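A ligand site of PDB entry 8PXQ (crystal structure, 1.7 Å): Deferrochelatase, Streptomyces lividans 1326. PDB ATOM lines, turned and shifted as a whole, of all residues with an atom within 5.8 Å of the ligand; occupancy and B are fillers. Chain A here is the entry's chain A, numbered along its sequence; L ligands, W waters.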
ATOM      1  N   ASN A 233     -25.273  -9.651  11.188  1.00  0.00           N
ATOM      2  CA  ASN A 233     -24.283  -8.620  10.947  1.00  0.00           C
ATOM      3  C   ASN A 233     -24.981  -7.386  10.338  1.00  0.00           C
ATOM      4  O   ASN A 233     -26.191  -7.403  10.106  1.00  0.00           O
ATOM      5  CB  ASN A 233     -23.112  -9.192  10.146  1.00  0.00           C
ATOM      6  CG  ASN A 233     -23.534  -9.737   8.808  1.00  0.00           C
ATOM      7  OD1 ASN A 233     -24.373  -9.121   8.155  1.00  0.00           O
ATOM      8  ND2 ASN A 233     -23.039 -10.925   8.448  1.00  0.00           N
ATOM      9  N   LEU A 235     -24.849  -6.252   7.423  1.00  0.00           N
ATOM     10  CA  LEU A 235     -25.411  -6.483   6.108  1.00  0.00           C
ATOM     11  C   LEU A 235     -26.792  -7.129   6.184  1.00  0.00           C
ATOM     12  O   LEU A 235     -27.457  -7.328   5.161  1.00  0.00           O
ATOM     13  CB  LEU A 235     -24.480  -7.351   5.304  1.00  0.00           C
ATOM     14  CG  LEU A 235     -23.058  -6.846   5.049  1.00  0.00           C
ATOM     15  CD1 LEU A 235     -22.333  -7.724   4.021  1.00  0.00           C
ATOM     16  CD2 LEU A 235     -23.098  -5.410   4.531  1.00  0.00           C
ATOM     17  N   PHE A 237     -27.617 -10.165   7.439  1.00  0.00           N
ATOM     18  CA  PHE A 237     -27.589 -11.636   7.342  1.00  0.00           C
ATOM     19  C   PHE A 237     -27.187 -12.226   8.685  1.00  0.00           C
ATOM     20  O   PHE A 237     -26.336 -11.695   9.388  1.00  0.00           O
ATOM     21  CB  PHE A 237     -26.674 -12.194   6.251  1.00  0.00           C
ATOM     22  CG  PHE A 237     -27.252 -12.134   4.870  1.00  0.00           C
ATOM     23  CD1 PHE A 237     -27.314 -10.920   4.167  1.00  0.00           C
ATOM     24  CD2 PHE A 237     -27.726 -13.286   4.204  1.00  0.00           C
ATOM     25  CE1 PHE A 237     -27.914 -10.818   2.920  1.00  0.00           C
ATOM     26  CE2 PHE A 237     -28.322 -13.147   2.953  1.00  0.00           C
ATOM     27  CZ  PHE A 237     -28.389 -11.951   2.306  1.00  0.00           C
ATOM     28  N   LYS A 238     -27.854 -13.355   9.026  1.00  0.00           N
ATOM     29  CA  LYS A 238     -27.412 -14.169  10.166  1.00  0.00           C
ATOM     30  C   LYS A 238     -25.980 -14.573   9.937  1.00  0.00           C
ATOM     31  O   LYS A 238     -25.624 -14.962   8.825  1.00  0.00           O
ATOM     32  CB  LYS A 238     -28.271 -15.448  10.299  1.00  0.00           C
ATOM     33  CG  LYS A 238     -29.722 -15.172  10.660  1.00  0.00           C
ATOM     34  CD  LYS A 238     -30.569 -16.420  10.675  1.00  0.00           C
ATOM     35  CE  LYS A 238     -31.973 -16.205  11.199  1.00  0.00           C
ATOM     36  NZ  LYS A 238     -32.833 -17.420  11.003  1.00  0.00           N
ATOM     37  N   ASP A 239     -25.205 -14.537  10.988  1.00  0.00           N
ATOM     38  CA  ASP A 239     -23.779 -14.818  10.951  1.00  0.00           C
ATOM     39  C   ASP A 239     -23.417 -15.673  12.154  1.00  0.00           C
ATOM     40  O   ASP A 239     -23.586 -15.192  13.278  1.00  0.00           O
ATOM     41  CB  ASP A 239     -23.020 -13.467  10.859  1.00  0.00           C
ATOM     42  CG  ASP A 239     -21.610 -13.562  10.313  1.00  0.00           C
ATOM     43  OD1 ASP A 239     -21.067 -14.708  10.192  1.00  0.00           O
ATOM     44  OD2 ASP A 239     -21.162 -12.487   9.822  1.00  0.00           O
ATOM     45  N   GLY A 240     -23.071 -16.968  11.890  1.00  0.00           N
ATOM     46  CA  GLY A 240     -22.651 -17.918  12.895  1.00  0.00           C
ATOM     47  C   GLY A 240     -23.428 -19.233  12.842  1.00  0.00           C
ATOM     48  O   GLY A 240     -23.291 -20.009  13.764  1.00  0.00           O
ATOM     49  N   THR A 241     -24.268 -19.419  11.830  1.00  0.00           N
ATOM     50  CA  THR A 241     -25.055 -20.643  11.707  1.00  0.00           C
ATOM     51  C   THR A 241     -24.191 -21.880  11.787  1.00  0.00           C
ATOM     52  O   THR A 241     -24.452 -22.780  12.586  1.00  0.00           O
ATOM     53  CB  THR A 241     -25.943 -20.664  10.454  1.00  0.00           C
ATOM     54  OG1 THR A 241     -26.777 -19.509  10.551  1.00  0.00           O
ATOM     55  CG2 THR A 241     -26.771 -21.952  10.360  1.00  0.00           C
ATOM     56  N   ARG A 242     -23.192 -21.947  10.874  1.00  0.00           N
ATOM     57  CA  ARG A 242     -22.313 -23.102  10.765  1.00  0.00           C
ATOM     58  C   ARG A 242     -20.950 -22.797  11.359  1.00  0.00           C
ATOM     59  O   ARG A 242     -20.037 -22.517  10.635  1.00  0.00           O
ATOM     60  CB  ARG A 242     -22.249 -23.563   9.316  1.00  0.00           C
ATOM     61  CG  ARG A 242     -23.361 -24.562   9.051  1.00  0.00           C
ATOM     62  CD  ARG A 242     -23.423 -25.183   7.711  1.00  0.00           C
ATOM     63  NE  ARG A 242     -22.144 -25.549   7.219  1.00  0.00           N
ATOM     64  CZ  ARG A 242     -21.412 -26.537   7.680  1.00  0.00           C
ATOM     65  NH1 ARG A 242     -20.117 -26.536   7.423  1.00  0.00           N
ATOM     66  NH2 ARG A 242     -21.995 -27.529   8.368  1.00  0.00           N
ATOM     67  N   ASN A 243     -20.862 -22.845  12.660  1.00  0.00           N
ATOM     68  CA  ASN A 243     -19.666 -22.540  13.416  1.00  0.00           C
ATOM     69  C   ASN A 243     -19.292 -23.828  14.152  1.00  0.00           C
ATOM     70  O   ASN A 243     -19.437 -24.930  13.582  1.00  0.00           O
ATOM     71  CB  ASN A 243     -19.894 -21.326  14.281  1.00  0.00           C
ATOM     72  CG  ASN A 243     -18.644 -20.625  14.727  1.00  0.00           C
ATOM     73  OD1 ASN A 243     -17.655 -20.604  13.993  1.00  0.00           O
ATOM     74  ND2 ASN A 243     -18.638 -20.103  15.928  1.00  0.00           N
ATOM     75  N   ARG A 276      -9.212  -9.579  12.125  1.00  0.00           N
ATOM     76  CA  ARG A 276      -9.254  -8.770  10.919  1.00  0.00           C
ATOM     77  C   ARG A 276     -10.323  -7.709  11.099  1.00  0.00           C
ATOM     78  O   ARG A 276     -11.481  -7.996  11.351  1.00  0.00           O
ATOM     79  CB  ARG A 276      -9.569  -9.596   9.685  1.00  0.00           C
ATOM     80  CG  ARG A 276      -8.601 -10.740   9.405  1.00  0.00           C
ATOM     81  CD  ARG A 276      -7.245 -10.308   8.905  1.00  0.00           C
ATOM     82  NE  ARG A 276      -7.365  -9.935   7.504  1.00  0.00           N
ATOM     83  CZ  ARG A 276      -6.367  -9.780   6.657  1.00  0.00           C
ATOM     84  NH1 ARG A 276      -5.107  -9.954   7.071  1.00  0.00           N
ATOM     85  NH2 ARG A 276      -6.654  -9.443   5.381  1.00  0.00           N
ATOM     86  N   ILE A 278     -12.631  -5.314   9.310  1.00  0.00           N
ATOM     87  CA  ILE A 278     -13.153  -5.294   7.955  1.00  0.00           C
ATOM     88  C   ILE A 278     -14.218  -4.189   7.825  1.00  0.00           C
ATOM     89  O   ILE A 278     -15.240  -4.172   8.515  1.00  0.00           O
ATOM     90  CB  ILE A 278     -13.787  -6.680   7.642  1.00  0.00           C
ATOM     91  CG1 ILE A 278     -12.810  -7.834   7.880  1.00  0.00           C
ATOM     92  CG2 ILE A 278     -14.318  -6.646   6.231  1.00  0.00           C
ATOM     93  CD1 ILE A 278     -13.355  -9.212   7.644  1.00  0.00           C
ATOM     94  N   MET A 280     -17.174  -2.292   5.863  1.00  0.00           N
ATOM     95  CA  MET A 280     -18.243  -2.684   4.939  1.00  0.00           C
ATOM     96  C   MET A 280     -18.597  -1.462   4.117  1.00  0.00           C
ATOM     97  O   MET A 280     -18.784  -0.396   4.701  1.00  0.00           O
ATOM     98  CB  MET A 280     -19.474  -3.245   5.676  1.00  0.00           C
ATOM     99  CG  MET A 280     -19.189  -4.530   6.379  1.00  0.00           C
ATOM    100  SD  MET A 280     -20.555  -4.844   7.538  1.00  0.00           S
ATOM    101  CE  MET A 280     -20.356  -6.615   7.568  1.00  0.00           C
ATOM    102  N   PHE A 297     -24.163 -14.530  -0.773  1.00  0.00           N
ATOM    103  CA  PHE A 297     -23.901 -15.424   0.335  1.00  0.00           C
ATOM    104  C   PHE A 297     -24.246 -16.897   0.005  1.00  0.00           C
ATOM    105  O   PHE A 297     -23.573 -17.776   0.502  1.00  0.00           O
ATOM    106  CB  PHE A 297     -24.677 -14.982   1.587  1.00  0.00           C
ATOM    107  CG  PHE A 297     -24.008 -13.816   2.266  1.00  0.00           C
ATOM    108  CD1 PHE A 297     -22.740 -13.972   2.831  1.00  0.00           C
ATOM    109  CD2 PHE A 297     -24.630 -12.594   2.322  1.00  0.00           C
ATOM    110  CE1 PHE A 297     -22.064 -12.888   3.338  1.00  0.00           C
ATOM    111  CE2 PHE A 297     -23.948 -11.490   2.868  1.00  0.00           C
ATOM    112  CZ  PHE A 297     -22.678 -11.665   3.382  1.00  0.00           C
ATOM    113  N   ARG A 299     -27.309 -17.970   0.917  1.00  0.00           N
ATOM    114  CA  ARG A 299     -28.414 -18.198   1.832  1.00  0.00           C
ATOM    115  C   ARG A 299     -29.413 -17.077   1.628  1.00  0.00           C
ATOM    116  O   ARG A 299     -29.048 -15.982   1.160  1.00  0.00           O
ATOM    117  CB  ARG A 299     -27.935 -18.194   3.287  1.00  0.00           C
ATOM    118  CG  ARG A 299     -27.068 -19.377   3.663  1.00  0.00           C
ATOM    119  CD  ARG A 299     -26.622 -19.310   5.067  1.00  0.00           C
ATOM    120  NE  ARG A 299     -25.893 -20.491   5.503  1.00  0.00           N
ATOM    121  CZ  ARG A 299     -26.454 -21.557   6.098  1.00  0.00           C
ATOM    122  NH1 ARG A 299     -27.769 -21.660   6.369  1.00  0.00           N
ATOM    123  NH2 ARG A 299     -25.614 -22.482   6.542  1.00  0.00           N
ATOM    124  N   PRO A 316     -26.203 -26.960   3.773  1.00  0.00           N
ATOM    125  CA  PRO A 316     -26.047 -26.374   2.445  1.00  0.00           C
ATOM    126  C   PRO A 316     -25.865 -27.457   1.397  1.00  0.00           C
ATOM    127  O   PRO A 316     -25.182 -28.484   1.643  1.00  0.00           O
ATOM    128  CB  PRO A 316     -24.815 -25.507   2.550  1.00  0.00           C
ATOM    129  CG  PRO A 316     -24.306 -25.621   3.872  1.00  0.00           C
ATOM    130  CD  PRO A 316     -25.202 -26.480   4.735  1.00  0.00           C
ATOM    131  N   HIS A 326     -20.163 -16.693  -1.039  1.00  0.00           N
ATOM    132  CA  HIS A 326     -19.347 -16.721   0.163  1.00  0.00           C
ATOM    133  C   HIS A 326     -19.407 -18.069   0.885  1.00  0.00           C
ATOM    134  O   HIS A 326     -18.365 -18.596   1.272  1.00  0.00           O
ATOM    135  CB  HIS A 326     -19.760 -15.565   1.070  1.00  0.00           C
ATOM    136  CG  HIS A 326     -18.944 -15.463   2.324  1.00  0.00           C
ATOM    137  ND1 HIS A 326     -17.635 -14.960   2.360  1.00  0.00           N
ATOM    138  CD2 HIS A 326     -19.290 -15.799   3.602  1.00  0.00           C
ATOM    139  CE1 HIS A 326     -17.227 -15.000   3.611  1.00  0.00           C
ATOM    140  NE2 HIS A 326     -18.221 -15.474   4.394  1.00  0.00           N
ATOM    141  N   VAL A 327     -20.586 -18.589   1.140  1.00  0.00           N
ATOM    142  CA  VAL A 327     -20.733 -19.834   1.880  1.00  0.00           C
ATOM    143  C   VAL A 327     -20.112 -20.963   1.088  1.00  0.00           C
ATOM    144  O   VAL A 327     -19.397 -21.780   1.669  1.00  0.00           O
ATOM    145  CB  VAL A 327     -22.189 -20.152   2.194  1.00  0.00           C
ATOM    146  CG1 VAL A 327     -22.349 -21.563   2.691  1.00  0.00           C
ATOM    147  CG2 VAL A 327     -22.672 -19.148   3.223  1.00  0.00           C
ATOM    148  N   ALA A 330     -16.289 -20.621   1.543  1.00  0.00           N
ATOM    149  CA  ALA A 330     -15.719 -20.694   2.892  1.00  0.00           C
ATOM    150  C   ALA A 330     -15.965 -22.034   3.559  1.00  0.00           C
ATOM    151  O   ALA A 330     -15.339 -22.333   4.562  1.00  0.00           O
ATOM    152  CB  ALA A 330     -16.377 -19.603   3.759  1.00  0.00           C
ATOM    153  N   HIS A 331     -16.886 -22.812   3.004  1.00  0.00           N
ATOM    154  CA  HIS A 331     -17.327 -24.085   3.588  1.00  0.00           C
ATOM    155  C   HIS A 331     -16.161 -25.066   3.726  1.00  0.00           C
ATOM    156  O   HIS A 331     -15.290 -25.118   2.865  1.00  0.00           O
ATOM    157  CB  HIS A 331     -18.380 -24.714   2.682  1.00  0.00           C
ATOM    158  CG  HIS A 331     -19.137 -25.869   3.302  1.00  0.00           C
ATOM    159  ND1 HIS A 331     -18.648 -27.149   3.442  1.00  0.00           N
ATOM    160  CD2 HIS A 331     -20.397 -25.925   3.783  1.00  0.00           C
ATOM    161  CE1 HIS A 331     -19.569 -27.907   4.031  1.00  0.00           C
ATOM    162  NE2 HIS A 331     -20.669 -27.190   4.225  1.00  0.00           N
ATOM    163  N   PRO A 332     -16.061 -25.824   4.812  1.00  0.00           N
ATOM    164  CA  PRO A 332     -14.938 -26.772   4.975  1.00  0.00           C
ATOM    165  C   PRO A 332     -14.759 -27.729   3.789  1.00  0.00           C
ATOM    166  O   PRO A 332     -13.596 -27.994   3.457  1.00  0.00           O
ATOM    167  CB  PRO A 332     -15.386 -27.506   6.250  1.00  0.00           C
ATOM    168  CG  PRO A 332     -16.085 -26.464   7.078  1.00  0.00           C
ATOM    169  CD  PRO A 332     -16.887 -25.727   6.031  1.00  0.00           C
ATOM    170  N   LEU A 340     -13.103 -23.352  11.240  1.00  0.00           N
ATOM    171  CA  LEU A 340     -12.710 -22.234  12.071  1.00  0.00           C
ATOM    172  C   LEU A 340     -13.756 -22.030  13.150  1.00  0.00           C
ATOM    173  O   LEU A 340     -14.909 -22.310  12.919  1.00  0.00           O
ATOM    174  CB  LEU A 340     -12.726 -20.913  11.278  1.00  0.00           C
ATOM    175  CG  LEU A 340     -11.828 -20.802  10.080  1.00  0.00           C
ATOM    176  CD1 LEU A 340     -12.018 -19.451   9.420  1.00  0.00           C
ATOM    177  CD2 LEU A 340     -10.407 -20.951  10.527  1.00  0.00           C
ATOM    178  N   ARG A 342     -15.452 -18.949  14.523  1.00  0.00           N
ATOM    179  CA  ARG A 342     -15.632 -17.538  14.361  1.00  0.00           C
ATOM    180  C   ARG A 342     -16.288 -16.929  15.578  1.00  0.00           C
ATOM    181  O   ARG A 342     -17.239 -17.472  16.121  1.00  0.00           O
ATOM    182  CB  ARG A 342     -16.481 -17.312  13.126  1.00  0.00           C
ATOM    183  CG  ARG A 342     -15.813 -17.737  11.838  1.00  0.00           C
ATOM    184  CD  ARG A 342     -16.745 -17.612  10.676  1.00  0.00           C
ATOM    185  NE  ARG A 342     -17.747 -18.659  10.695  1.00  0.00           N
ATOM    186  CZ  ARG A 342     -19.038 -18.534  10.436  1.00  0.00           C
ATOM    187  NH1 ARG A 342     -19.547 -17.362  10.096  1.00  0.00           N
ATOM    188  NH2 ARG A 342     -19.748 -19.624  10.538  1.00  0.00           N
ATOM    189  N   LEU A 361     -17.103  -5.021  10.556  1.00  0.00           N
ATOM    190  CA  LEU A 361     -17.084  -6.289  11.277  1.00  0.00           C
ATOM    191  C   LEU A 361     -15.653  -6.494  11.735  1.00  0.00           C
ATOM    192  O   LEU A 361     -14.715  -6.469  10.967  1.00  0.00           O
ATOM    193  CB  LEU A 361     -17.622  -7.431  10.389  1.00  0.00           C
ATOM    194  CG  LEU A 361     -18.101  -8.673  11.069  1.00  0.00           C
ATOM    195  CD1 LEU A 361     -19.189  -9.400  10.278  1.00  0.00           C
ATOM    196  CD2 LEU A 361     -16.952  -9.593  11.286  1.00  0.00           C
ATOM    197  N   PHE A 363     -13.617  -9.193  12.740  1.00  0.00           N
ATOM    198  CA  PHE A 363     -13.614 -10.636  12.543  1.00  0.00           C
ATOM    199  C   PHE A 363     -12.556 -11.264  13.445  1.00  0.00           C
ATOM    200  O   PHE A 363     -11.395 -10.852  13.468  1.00  0.00           O
ATOM    201  CB  PHE A 363     -13.318 -10.865  11.053  1.00  0.00           C
ATOM    202  CG  PHE A 363     -13.355 -12.342  10.707  1.00  0.00           C
ATOM    203  CD1 PHE A 363     -14.572 -12.943  10.418  1.00  0.00           C
ATOM    204  CD2 PHE A 363     -12.194 -13.099  10.705  1.00  0.00           C
ATOM    205  CE1 PHE A 363     -14.608 -14.313  10.090  1.00  0.00           C
ATOM    206  CE2 PHE A 363     -12.256 -14.465  10.419  1.00  0.00           C
ATOM    207  CZ  PHE A 363     -13.439 -15.042  10.052  1.00  0.00           C
ATOM    208  N   PHE A 374      -7.401 -20.272   9.103  1.00  0.00           N
ATOM    209  CA  PHE A 374      -7.707 -18.997   8.428  1.00  0.00           C
ATOM    210  C   PHE A 374      -7.039 -18.878   7.051  1.00  0.00           C
ATOM    211  O   PHE A 374      -7.635 -18.448   6.095  1.00  0.00           O
ATOM    212  CB  PHE A 374      -7.303 -17.804   9.281  1.00  0.00           C
ATOM    213  CG  PHE A 374      -7.575 -16.457   8.651  1.00  0.00           C
ATOM    214  CD1 PHE A 374      -8.841 -15.908   8.662  1.00  0.00           C
ATOM    215  CD2 PHE A 374      -6.559 -15.788   7.940  1.00  0.00           C
ATOM    216  CE1 PHE A 374      -9.072 -14.672   8.060  1.00  0.00           C
ATOM    217  CE2 PHE A 374      -6.798 -14.553   7.350  1.00  0.00           C
ATOM    218  CZ  PHE A 374      -8.057 -14.008   7.407  1.00  0.00           C
ATOM    219  N   VAL A 377      -8.743 -20.819   4.070  1.00  0.00           N
ATOM    220  CA  VAL A 377     -10.066 -20.303   3.844  1.00  0.00           C
ATOM    221  C   VAL A 377      -9.975 -18.924   3.187  1.00  0.00           C
ATOM    222  O   VAL A 377     -10.638 -18.668   2.181  1.00  0.00           O
ATOM    223  CB  VAL A 377     -10.959 -20.372   5.116  1.00  0.00           C
ATOM    224  CG1 VAL A 377     -12.327 -19.755   4.842  1.00  0.00           C
ATOM    225  CG2 VAL A 377     -11.095 -21.796   5.646  1.00  0.00           C
ATOM    226  N   GLN A 378      -9.235 -17.985   3.786  1.00  0.00           N
ATOM    227  CA  GLN A 378      -9.184 -16.653   3.184  1.00  0.00           C
ATOM    228  C   GLN A 378      -8.565 -16.656   1.799  1.00  0.00           C
ATOM    229  O   GLN A 378      -8.945 -15.880   0.945  1.00  0.00           O
ATOM    230  CB  GLN A 378      -8.330 -15.759   4.120  1.00  0.00           C
ATOM    231  CG  GLN A 378      -8.143 -14.340   3.624  1.00  0.00           C
ATOM    232  CD  GLN A 378      -9.412 -13.521   3.482  1.00  0.00           C
ATOM    233  OE1 GLN A 378     -10.366 -13.680   4.238  1.00  0.00           O
ATOM    234  NE2 GLN A 378      -9.490 -12.643   2.504  1.00  0.00           N
ATOM    235  N   LEU A 381     -11.147 -17.243  -0.563  1.00  0.00           N
ATOM    236  CA  LEU A 381     -12.079 -16.150  -0.732  1.00  0.00           C
ATOM    237  C   LEU A 381     -11.602 -15.115  -1.753  1.00  0.00           C
ATOM    238  O   LEU A 381     -12.227 -14.059  -1.881  1.00  0.00           O
ATOM    239  CB  LEU A 381     -12.426 -15.507   0.601  1.00  0.00           C
ATOM    240  CG  LEU A 381     -13.080 -16.435   1.646  1.00  0.00           C
ATOM    241  CD1 LEU A 381     -13.398 -15.591   2.910  1.00  0.00           C
ATOM    242  CD2 LEU A 381     -14.328 -17.108   1.136  1.00  0.00           C
ATOM    243  N   LEU A 386     -18.427 -11.385  -2.080  1.00  0.00           N
ATOM    244  CA  LEU A 386     -18.524 -10.437  -0.967  1.00  0.00           C
ATOM    245  C   LEU A 386     -17.408  -9.383  -1.063  1.00  0.00           C
ATOM    246  O   LEU A 386     -17.544  -8.306  -0.513  1.00  0.00           O
ATOM    247  CB  LEU A 386     -18.462 -11.233   0.330  1.00  0.00           C
ATOM    248  CG  LEU A 386     -18.547 -10.426   1.636  1.00  0.00           C
ATOM    249  CD1 LEU A 386     -19.863  -9.736   1.726  1.00  0.00           C
ATOM    250  CD2 LEU A 386     -18.360 -11.381   2.826  1.00  0.00           C
ATOM    251  N   ILE A 390     -16.549  -5.237   0.856  1.00  0.00           N
ATOM    252  CA  ILE A 390     -15.769  -5.205   2.089  1.00  0.00           C
ATOM    253  C   ILE A 390     -14.352  -4.788   1.773  1.00  0.00           C
ATOM    254  O   ILE A 390     -13.905  -4.923   0.622  1.00  0.00           O
ATOM    255  CB  ILE A 390     -15.813  -6.558   2.822  1.00  0.00           C
ATOM    256  CG1 ILE A 390     -15.160  -7.691   2.017  1.00  0.00           C
ATOM    257  CG2 ILE A 390     -17.250  -6.911   3.241  1.00  0.00           C
ATOM    258  CD1 ILE A 390     -14.820  -8.946   2.767  1.00  0.00           C
ATOM    259  N   HIS A 392     -10.517  -5.337   4.013  1.00  0.00           N
ATOM    260  CA  HIS A 392      -9.770  -5.631   5.217  1.00  0.00           C
ATOM    261  C   HIS A 392      -8.822  -4.467   5.460  1.00  0.00           C
ATOM    262  O   HIS A 392      -7.994  -4.198   4.593  1.00  0.00           O
ATOM    263  CB  HIS A 392      -8.987  -6.927   5.102  1.00  0.00           C
ATOM    264  CG  HIS A 392      -9.816  -8.165   5.018  1.00  0.00           C
ATOM    265  ND1 HIS A 392      -9.697  -9.225   5.908  1.00  0.00           N
ATOM    266  CD2 HIS A 392     -10.809  -8.506   4.157  1.00  0.00           C
ATOM    267  CE1 HIS A 392     -10.543 -10.178   5.544  1.00  0.00           C
ATOM    268  NE2 HIS A 392     -11.259  -9.767   4.454  1.00  0.00           N
HETATM  269  C1  LIG L   1     -20.312 -18.026   6.780  1.00  0.00           C
HETATM  270  C2  LIG L   1     -20.922 -13.250   6.413  1.00  0.00           C
HETATM  271  C3  LIG L   1     -16.139 -12.687   6.539  1.00  0.00           C
HETATM  272  C4  LIG L   1     -15.593 -17.534   6.986  1.00  0.00           C
HETATM  273  C5  LIG L   1     -20.897 -16.771   6.642  1.00  0.00           C
HETATM  274  C6  LIG L   1     -22.309 -16.559   6.581  1.00  0.00           C
HETATM  275  C7  LIG L   1     -22.470 -15.219   6.486  1.00  0.00           C
HETATM  276  C8  LIG L   1     -21.195 -14.623   6.471  1.00  0.00           C
HETATM  277  C9  LIG L   1     -23.801 -14.445   6.375  1.00  0.00           C
HETATM  278  C10 LIG L   1     -23.488 -17.558   6.553  1.00  0.00           C
HETATM  279  C11 LIG L   1     -23.998 -18.052   7.941  1.00  0.00           C
HETATM  280  C12 LIG L   1     -22.913 -18.779   8.691  1.00  0.00           C
HETATM  281  O1  LIG L   1     -22.231 -18.163   9.509  1.00  0.00           O
HETATM  282  O2  LIG L   1     -22.795 -20.037   8.551  1.00  0.00           O
HETATM  283  C13 LIG L   1     -19.652 -12.703   6.494  1.00  0.00           C
HETATM  284  C14 LIG L   1     -19.395 -11.277   6.413  1.00  0.00           C
HETATM  285  C15 LIG L   1     -18.029 -11.099   6.394  1.00  0.00           C
HETATM  286  C16 LIG L   1     -17.481 -12.440   6.485  1.00  0.00           C
HETATM  287  C17 LIG L   1     -20.436 -10.259   6.352  1.00  0.00           C
HETATM  288  C18 LIG L   1     -17.200  -9.884   6.485  1.00  0.00           C
HETATM  289  C19 LIG L   1     -17.639  -8.678   6.671  1.00  0.00           C
HETATM  290  C20 LIG L   1     -15.522 -13.943   6.647  1.00  0.00           C
HETATM  291  C21 LIG L   1     -14.141 -14.181   6.626  1.00  0.00           C
HETATM  292  C22 LIG L   1     -14.019 -15.510   6.807  1.00  0.00           C
HETATM  293  C23 LIG L   1     -15.302 -16.150   6.830  1.00  0.00           C
HETATM  294  C24 LIG L   1     -13.038 -13.151   6.614  1.00  0.00           C
HETATM  295  C25 LIG L   1     -12.902 -16.392   6.843  1.00  0.00           C
HETATM  296  C26 LIG L   1     -11.722 -16.147   6.321  1.00  0.00           C
HETATM  297  C27 LIG L   1     -16.865 -18.026   7.035  1.00  0.00           C
HETATM  298  C28 LIG L   1     -17.133 -19.485   7.209  1.00  0.00           C
HETATM  299  C29 LIG L   1     -18.490 -19.584   7.162  1.00  0.00           C
HETATM  300  C30 LIG L   1     -18.968 -18.241   6.889  1.00  0.00           C
HETATM  301  C31 LIG L   1     -16.059 -20.522   7.461  1.00  0.00           C
HETATM  302  C32 LIG L   1     -19.261 -20.860   7.295  1.00  0.00           C
HETATM  303  C33 LIG L   1     -19.314 -21.651   5.981  1.00  0.00           C
HETATM  304  C34 LIG L   1     -19.988 -22.992   6.216  1.00  0.00           C
HETATM  305  O3  LIG L   1     -21.195 -23.204   5.895  1.00  0.00           O
HETATM  306  O4  LIG L   1     -19.352 -23.905   6.772  1.00  0.00           O
HETATM  307  N1  LIG L   1     -20.217 -15.547   6.565  1.00  0.00           N
HETATM  308  N2  LIG L   1     -18.467 -13.316   6.553  1.00  0.00           N
HETATM  309  N3  LIG L   1     -16.191 -15.136   6.743  1.00  0.00           N
HETATM  310  N4  LIG L   1     -17.982 -17.349   6.848  1.00  0.00           N
HETATM  311 FE1  LIG L   1     -18.223 -15.374   6.532  1.00  0.00          FE
HETATM  312  O   HOH W   1     -15.505 -23.141   9.423  1.00  0.00           O
HETATM  313  O   HOH W   2     -23.077 -21.228   6.237  1.00  0.00           O
HETATM  314  O   HOH W   3     -14.233 -23.213   6.927  1.00  0.00           O
HETATM  315  O   HOH W   4     -12.572 -11.911   3.392  1.00  0.00           O
HETATM  316  O   HOH W   5     -18.482 -12.518   9.748  1.00  0.00           O
HETATM  317  O   HOH W   6     -18.171 -23.979   9.230  1.00  0.00           O
HETATM  318  O   HOH W   7     -18.566 -14.973   8.881  1.00  0.00           O
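An iron atom (FE1) of the ligand is bound by a ring nitrogen (NE2) of His 326, 2.1 Å away.
The backbone NH (N) of Gly 240 is in hydrogen-bond range of an oxygen (O1) of the ligand.
The backbone NH (N) of Arg 242 lies within hydrogen-bond range of an oxygen (O2) of the ligand (3.0 Å).
The guanidinium group (NH1) of Arg 242 is in salt-bridge range of an oxygen (O4) of the ligand, 2.8 Å away.
NH1 of Arg 342 lies within salt-bridge range of O1 of the ligand (2.9 Å).
The backbone NH (N) of Thr 241 is in hydrogen-bond range of an oxygen (O1) of the ligand, 3.3 Å away.
O of Arg 242 is in hydrogen-bond range of NH2 of Arg 342.
NH1 of Arg 242 sits at hydrogen-bond distance from NE2 of His 331 (3.3 Å).
NH1 of Arg 342 is in salt-bridge range of OD1 of Asp 239, at 3.1 Å.
N of Arg 342 is in hydrogen-bond range of OD1 of Asn 243, 2.8 Å away.
N of Phe 363 lies within hydrogen-bond range of O of Arg 276, at 2.8 Å.
The side-chain amide nitrogen of Asn 233 lies within hydrogen-bond range of the side-chain carboxylate of Asp 239, 2.8 Å away.
The side-chain amide oxygen (OD1) of Asn 233 sits close to the backbone carbonyl oxygen (O) of Phe 237.
O of Ile 278 is in hydrogen-bond range of N of Leu 361, 2.9 Å away.
Merely in contact with the ligand: Lys 238 (3.1 Å), Pro 332 (3.2 Å), Phe 297 (3.3 Å), Phe 363 (3.3 Å), Asn 233 (3.4 Å), Ala 330 (3.5 Å), Phe 374 (3.5 Å), Asp 239 (3.5 Å), Gln 378 (3.5 Å), Met 280 (3.5 Å), His 331 (3.5 Å), Leu 386 (3.6 Å), Phe 237 (3.7 Å), Val 327 (3.8 Å), Leu 381 (3.8 Å), Ile 390 (3.9 Å), Arg 299 (3.9 Å), Ile 278 (3.9 Å), Leu 361 (3.9 Å), Leu 235 (3.9 Å) and Val 377 (3.9 Å).
Hydrophobic or aromatic side chains that line the ligand: Leu 235, Phe 237, Ile 278, Met 280, Phe 297, His 326, Val 327, Ala 330, His 331, Pro 332, Leu 361, Phe 363, Phe 374, Val 377, Leu 381, Leu 386 and Ile 390.
Within 4 Å of the ligand: Asn 233, Leu 235, Phe 237, Lys 238, Asp 239, Gly 240, Thr 241, Arg 242, Ile 278, Met 280, Phe 297, Arg 299, His 326, Val 327, Ala 330, His 331, Pro 332, Arg 342, Leu 361, Phe 363, Phe 374, Val 377, Gln 378, Leu 381, Leu 386 and Ile 390.
Along chain A the residues within 4 Å of the ligand span positions 233 to 390.
Water W7 lies within hydrogen-bond range of the side-chain carboxylate of Asp 239 (2.8 Å) and the guanidinium group of Arg 342 (2.9 Å).
Water W2 lies within hydrogen-bond range of O2 of the ligand (2.6 Å) and NH2 of Arg 299 (2.8 Å).
Water W6 lies within hydrogen-bond range of O4 of the ligand (2.7 Å) and O of Arg 242 (2.8 Å).
Water W4 lies within hydrogen-bond range of a ring nitrogen (NE2) of His 392 and the side-chain amide oxygen of Gln 378.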
